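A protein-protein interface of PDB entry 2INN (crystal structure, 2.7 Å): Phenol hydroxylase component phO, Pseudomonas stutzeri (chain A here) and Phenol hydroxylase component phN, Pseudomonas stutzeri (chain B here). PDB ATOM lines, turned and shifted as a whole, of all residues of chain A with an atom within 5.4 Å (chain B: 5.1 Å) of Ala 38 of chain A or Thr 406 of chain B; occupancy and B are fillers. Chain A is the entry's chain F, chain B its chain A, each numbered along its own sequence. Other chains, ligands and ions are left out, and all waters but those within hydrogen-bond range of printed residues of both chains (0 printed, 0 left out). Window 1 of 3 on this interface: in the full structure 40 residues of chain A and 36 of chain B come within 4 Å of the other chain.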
ATOM      1  N   VAL A  28      30.994  -1.565  16.377  1.00  0.00           N
ATOM      2  CA  VAL A  28      31.482  -2.732  15.706  1.00  0.00           C
ATOM      3  C   VAL A  28      30.357  -3.715  15.561  1.00  0.00           C
ATOM      4  O   VAL A  28      29.666  -4.120  16.578  1.00  0.00           O
ATOM      5  CB  VAL A  28      32.639  -3.500  16.410  1.00  0.00           C
ATOM      6  CG1 VAL A  28      33.285  -4.422  15.363  1.00  0.00           C
ATOM      7  CG2 VAL A  28      33.743  -2.619  16.917  1.00  0.00           C
ATOM      8  N   LEU A  34      24.557 -13.074  15.574  1.00  0.00           N
ATOM      9  CA  LEU A  34      23.456 -12.428  16.233  1.00  0.00           C
ATOM     10  C   LEU A  34      23.325 -12.785  17.713  1.00  0.00           C
ATOM     11  O   LEU A  34      22.604 -12.124  18.445  1.00  0.00           O
ATOM     12  CB  LEU A  34      22.162 -12.591  15.433  1.00  0.00           C
ATOM     13  CG  LEU A  34      22.389 -11.759  14.145  1.00  0.00           C
ATOM     14  CD1 LEU A  34      21.607 -12.287  12.975  1.00  0.00           C
ATOM     15  CD2 LEU A  34      22.030 -10.337  14.334  1.00  0.00           C
ATOM     16  N   PHE A  36      24.825 -11.756  19.913  1.00  0.00           N
ATOM     17  CA  PHE A  36      24.891 -10.352  20.322  1.00  0.00           C
ATOM     18  C   PHE A  36      23.905  -9.696  19.448  1.00  0.00           C
ATOM     19  O   PHE A  36      24.169  -9.492  18.240  1.00  0.00           O
ATOM     20  CB  PHE A  36      26.293  -9.734  20.045  1.00  0.00           C
ATOM     21  CG  PHE A  36      27.360 -10.541  20.587  1.00  0.00           C
ATOM     22  CD1 PHE A  36      28.120 -11.352  19.747  1.00  0.00           C
ATOM     23  CD2 PHE A  36      27.548 -10.615  21.980  1.00  0.00           C
ATOM     24  CE1 PHE A  36      29.136 -12.213  20.285  1.00  0.00           C
ATOM     25  CE2 PHE A  36      28.532 -11.499  22.537  1.00  0.00           C
ATOM     26  CZ  PHE A  36      29.322 -12.292  21.673  1.00  0.00           C
ATOM     27  N   CYS A  37      22.800  -9.357  20.077  1.00  0.00           N
ATOM     28  CA  CYS A  37      21.696  -8.866  19.365  1.00  0.00           C
ATOM     29  C   CYS A  37      21.990  -7.678  18.435  1.00  0.00           C
ATOM     30  O   CYS A  37      21.315  -7.512  17.418  1.00  0.00           O
ATOM     31  CB  CYS A  37      20.620  -8.500  20.352  1.00  0.00           C
ATOM     32  SG  CYS A  37      20.953  -7.069  21.411  1.00  0.00           S
ATOM     33  N   ALA A  38      22.965  -6.859  18.769  1.00  0.00           N
ATOM     34  CA  ALA A  38      23.165  -5.601  18.094  1.00  0.00           C
ATOM     35  C   ALA A  38      24.678  -5.249  18.080  1.00  0.00           C
ATOM     36  O   ALA A  38      25.475  -5.774  18.924  1.00  0.00           O
ATOM     37  CB  ALA A  38      22.372  -4.509  18.798  1.00  0.00           C
ATOM     38  N   PRO A  39      25.099  -4.383  17.127  1.00  0.00           N
ATOM     39  CA  PRO A  39      26.548  -4.012  17.087  1.00  0.00           C
ATOM     40  C   PRO A  39      26.919  -3.420  18.412  1.00  0.00           C
ATOM     41  O   PRO A  39      26.028  -2.775  19.058  1.00  0.00           O
ATOM     42  CB  PRO A  39      26.646  -2.945  15.967  1.00  0.00           C
ATOM     43  CG  PRO A  39      25.417  -3.239  15.080  1.00  0.00           C
ATOM     44  CD  PRO A  39      24.310  -3.739  16.064  1.00  0.00           C
ATOM     45  N   PHE A  40      28.176  -3.624  18.835  1.00  0.00           N
ATOM     46  CA  PHE A  40      28.643  -3.053  20.096  1.00  0.00           C
ATOM     47  C   PHE A  40      28.749  -1.559  20.043  1.00  0.00           C
ATOM     48  O   PHE A  40      29.025  -0.964  18.973  1.00  0.00           O
ATOM     49  CB  PHE A  40      30.010  -3.602  20.437  1.00  0.00           C
ATOM     50  CG  PHE A  40      30.025  -5.047  20.568  1.00  0.00           C
ATOM     51  CD1 PHE A  40      29.312  -5.676  21.628  1.00  0.00           C
ATOM     52  CD2 PHE A  40      30.705  -5.822  19.653  1.00  0.00           C
ATOM     53  CE1 PHE A  40      29.271  -7.084  21.769  1.00  0.00           C
ATOM     54  CE2 PHE A  40      30.680  -7.266  19.789  1.00  0.00           C
ATOM     55  CZ  PHE A  40      29.938  -7.893  20.827  1.00  0.00           C
ATOM     56  N   PRO B 396      24.830  -1.939  23.694  1.00  0.00           N
ATOM     57  CA  PRO B 396      24.529  -2.013  22.254  1.00  0.00           C
ATOM     58  C   PRO B 396      24.475  -0.644  21.682  1.00  0.00           C
ATOM     59  O   PRO B 396      24.149   0.365  22.406  1.00  0.00           O
ATOM     60  CB  PRO B 396      23.074  -2.519  22.218  1.00  0.00           C
ATOM     61  CG  PRO B 396      22.507  -2.083  23.518  1.00  0.00           C
ATOM     62  CD  PRO B 396      23.613  -1.789  24.505  1.00  0.00           C
ATOM     63  N   GLN B 397      24.738  -0.604  20.391  1.00  0.00           N
ATOM     64  CA  GLN B 397      24.378   0.556  19.622  1.00  0.00           C
ATOM     65  C   GLN B 397      22.843   0.860  19.661  1.00  0.00           C
ATOM     66  O   GLN B 397      22.043  -0.054  19.406  1.00  0.00           O
ATOM     67  CB  GLN B 397      24.811   0.299  18.201  1.00  0.00           C
ATOM     68  CG  GLN B 397      23.966   1.056  17.154  1.00  0.00           C
ATOM     69  CD  GLN B 397      24.659   1.140  15.799  1.00  0.00           C
ATOM     70  OE1 GLN B 397      24.387   0.336  14.888  1.00  0.00           O
ATOM     71  NE2 GLN B 397      25.585   2.105  15.670  1.00  0.00           N
ATOM     72  N   LEU B 398      22.452   2.122  19.946  1.00  0.00           N
ATOM     73  CA  LEU B 398      21.002   2.503  19.906  1.00  0.00           C
ATOM     74  C   LEU B 398      20.570   3.202  18.623  1.00  0.00           C
ATOM     75  O   LEU B 398      21.408   3.811  17.993  1.00  0.00           O
ATOM     76  CB  LEU B 398      20.606   3.432  21.065  1.00  0.00           C
ATOM     77  CG  LEU B 398      20.794   2.949  22.504  1.00  0.00           C
ATOM     78  CD1 LEU B 398      20.317   4.017  23.502  1.00  0.00           C
ATOM     79  CD2 LEU B 398      20.171   1.585  22.733  1.00  0.00           C
ATOM     80  N   CYS B 399      19.286   3.175  18.233  1.00  0.00           N
ATOM     81  CA  CYS B 399      18.883   3.829  16.989  1.00  0.00           C
ATOM     82  C   CYS B 399      18.608   5.306  17.282  1.00  0.00           C
ATOM     83  O   CYS B 399      17.897   5.606  18.245  1.00  0.00           O
ATOM     84  CB  CYS B 399      17.632   3.158  16.417  1.00  0.00           C
ATOM     85  SG  CYS B 399      16.931   4.141  14.995  1.00  0.00           S
ATOM     86  N   ILE B 404      15.683   2.047  20.243  1.00  0.00           N
ATOM     87  CA  ILE B 404      15.814   0.648  20.500  1.00  0.00           C
ATOM     88  C   ILE B 404      17.196   0.199  20.018  1.00  0.00           C
ATOM     89  O   ILE B 404      17.656   0.703  19.049  1.00  0.00           O
ATOM     90  CB  ILE B 404      14.806  -0.113  19.649  1.00  0.00           C
ATOM     91  CG1 ILE B 404      13.371   0.223  20.062  1.00  0.00           C
ATOM     92  CG2 ILE B 404      15.056  -1.607  19.783  1.00  0.00           C
ATOM     93  CD1 ILE B 404      12.230  -0.645  19.394  1.00  0.00           C
ATOM     94  N   PRO B 405      17.833  -0.813  20.647  1.00  0.00           N
ATOM     95  CA  PRO B 405      19.019  -1.342  19.987  1.00  0.00           C
ATOM     96  C   PRO B 405      18.794  -1.777  18.553  1.00  0.00           C
ATOM     97  O   PRO B 405      17.719  -2.266  18.216  1.00  0.00           O
ATOM     98  CB  PRO B 405      19.334  -2.564  20.818  1.00  0.00           C
ATOM     99  CG  PRO B 405      18.779  -2.252  22.123  1.00  0.00           C
ATOM    100  CD  PRO B 405      17.547  -1.528  21.907  1.00  0.00           C
ATOM    101  N   THR B 406      19.801  -1.605  17.715  1.00  0.00           N
ATOM    102  CA  THR B 406      19.736  -2.008  16.318  1.00  0.00           C
ATOM    103  C   THR B 406      19.762  -3.526  16.088  1.00  0.00           C
ATOM    104  O   THR B 406      20.671  -4.102  15.475  1.00  0.00           O
ATOM    105  CB  THR B 406      20.732  -1.217  15.381  1.00  0.00           C
ATOM    106  OG1 THR B 406      22.094  -1.402  15.794  1.00  0.00           O
ATOM    107  CG2 THR B 406      20.418   0.250  15.426  1.00  0.00           C
ATOM    108  N   ILE B 407      18.687  -4.169  16.529  1.00  0.00           N
ATOM    109  CA  ILE B 407      18.556  -5.634  16.498  1.00  0.00           C
ATOM    110  C   ILE B 407      17.731  -6.079  15.287  1.00  0.00           C
ATOM    111  O   ILE B 407      17.675  -7.295  14.931  1.00  0.00           O
ATOM    112  CB  ILE B 407      17.876  -6.089  17.732  1.00  0.00           C
ATOM    113  CG1 ILE B 407      16.588  -5.390  17.799  1.00  0.00           C
ATOM    114  CG2 ILE B 407      18.547  -5.552  18.922  1.00  0.00           C
ATOM    115  CD1 ILE B 407      15.851  -5.866  19.056  1.00  0.00           C
ATOM    116  N   PHE B 408      17.110  -5.116  14.622  1.00  0.00           N
ATOM    117  CA  PHE B 408      16.265  -5.468  13.524  1.00  0.00           C
ATOM    118  C   PHE B 408      16.941  -5.853  12.203  1.00  0.00           C
ATOM    119  O   PHE B 408      18.009  -5.338  11.834  1.00  0.00           O
ATOM    120  CB  PHE B 408      15.293  -4.358  13.377  1.00  0.00           C
ATOM    121  CG  PHE B 408      14.557  -4.069  14.620  1.00  0.00           C
ATOM    122  CD1 PHE B 408      14.644  -2.820  15.206  1.00  0.00           C
ATOM    123  CD2 PHE B 408      13.725  -5.032  15.171  1.00  0.00           C
ATOM    124  CE1 PHE B 408      13.894  -2.505  16.385  1.00  0.00           C
ATOM    125  CE2 PHE B 408      12.984  -4.790  16.322  1.00  0.00           C
ATOM    126  CZ  PHE B 408      13.063  -3.530  16.948  1.00  0.00           C
ATOM    127  N   LEU B 417      21.352  -7.710   9.858  1.00  0.00           N
ATOM    128  CA  LEU B 417      21.019  -6.528  10.510  1.00  0.00           C
ATOM    129  C   LEU B 417      20.704  -5.486   9.420  1.00  0.00           C
ATOM    130  O   LEU B 417      21.405  -5.359   8.416  1.00  0.00           O
ATOM    131  CB  LEU B 417      22.218  -6.183  11.385  1.00  0.00           C
ATOM    132  CG  LEU B 417      21.760  -6.029  12.821  1.00  0.00           C
ATOM    133  CD1 LEU B 417      20.645  -7.048  13.036  1.00  0.00           C
ATOM    134  CD2 LEU B 417      22.866  -6.251  13.772  1.00  0.00           C
ATOM    135  N   PHE B 431      20.842   4.206  12.532  1.00  0.00           N
ATOM    136  CA  PHE B 431      19.428   3.893  12.419  1.00  0.00           C
ATOM    137  C   PHE B 431      19.156   2.411  12.376  1.00  0.00           C
ATOM    138  O   PHE B 431      19.851   1.622  11.679  1.00  0.00           O
ATOM    139  CB  PHE B 431      18.817   4.590  11.157  1.00  0.00           C
ATOM    140  CG  PHE B 431      19.016   6.042  11.184  1.00  0.00           C
ATOM    141  CD1 PHE B 431      18.386   6.792  12.167  1.00  0.00           C
ATOM    142  CD2 PHE B 431      19.980   6.601  10.392  1.00  0.00           C
ATOM    143  CE1 PHE B 431      18.671   8.125  12.306  1.00  0.00           C
ATOM    144  CE2 PHE B 431      20.299   7.917  10.490  1.00  0.00           C
ATOM    145  CZ  PHE B 431      19.633   8.709  11.439  1.00  0.00           C
ATOM    146  N   CYS B 432      18.103   2.042  13.090  1.00  0.00           N
ATOM    147  CA  CYS B 432      17.593   0.696  13.042  1.00  0.00           C
ATOM    148  C   CYS B 432      17.071   0.227  11.677  1.00  0.00           C
ATOM    149  O   CYS B 432      16.995  -0.954  11.478  1.00  0.00           O
ATOM    150  CB  CYS B 432      16.471   0.592  14.083  1.00  0.00           C
ATOM    151  SG  CYS B 432      14.998   1.114  13.483  1.00  0.00           S
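N of Gln 397 of chain B lies within hydrogen-bond range of O of Pro 39 of chain A (2.9 Å).
The side-chain amide oxygen (OE1) of Gln 397 of chain B sits at hydrogen-bond distance from the side-chain hydroxyl (OG1) of Thr 406 of chain B (3.0 Å).
Among the printed residues, merely in contact across the chains: Leu 34 of chain A with Leu 417 of chain B, Cys 37 of chain A with Thr 406 of chain B, Cys 37 of chain A with Ile 407 of chain B, Ala 38 of chain A with Thr 406 of chain B, Ala 38 of chain A with Ile 407 of chain B, Pro 39 of chain A with Pro 396 of chain B, Pro 39 of chain A with Thr 406 of chain B and Pro 39 of chain A with Leu 417 of chain B.
Of the printed residues of chain B, Leu 34 of chain A touches Leu 417 (3.8 Å). Of the printed residues of chain B, Cys 37 of chain A touches Thr 406 (3.98 Å) and Ile 407 (3.5 Å). Of the printed residues of chain B, Ala 38 of chain A touches Thr 406 and Ile 407. Printed residues of chain B within 4 Å of Pro 39 of chain A: Pro 396, Gln 397, Thr 406 and Leu 417. Of chain A, only Cys 37, Ala 38 and Pro 39 come within 4 Å of Thr 406 of chain B. Phe 408 of chain B touches none of the printed residues of chain A. Of the printed residues of chain A, Leu 417 of chain B touches Leu 34 (3.8 Å) and Pro 39 (3.7 Å).
Printed residues of chain A that touch a printed residue of chain B: Leu 34, Cys 37, Ala 38 and Pro 39. Hydrophobic or aromatic side chains of chain B that line the printed part of chain A: Ile 407 and Leu 417. Among the printed residues, 9 pairs touch across the chains.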
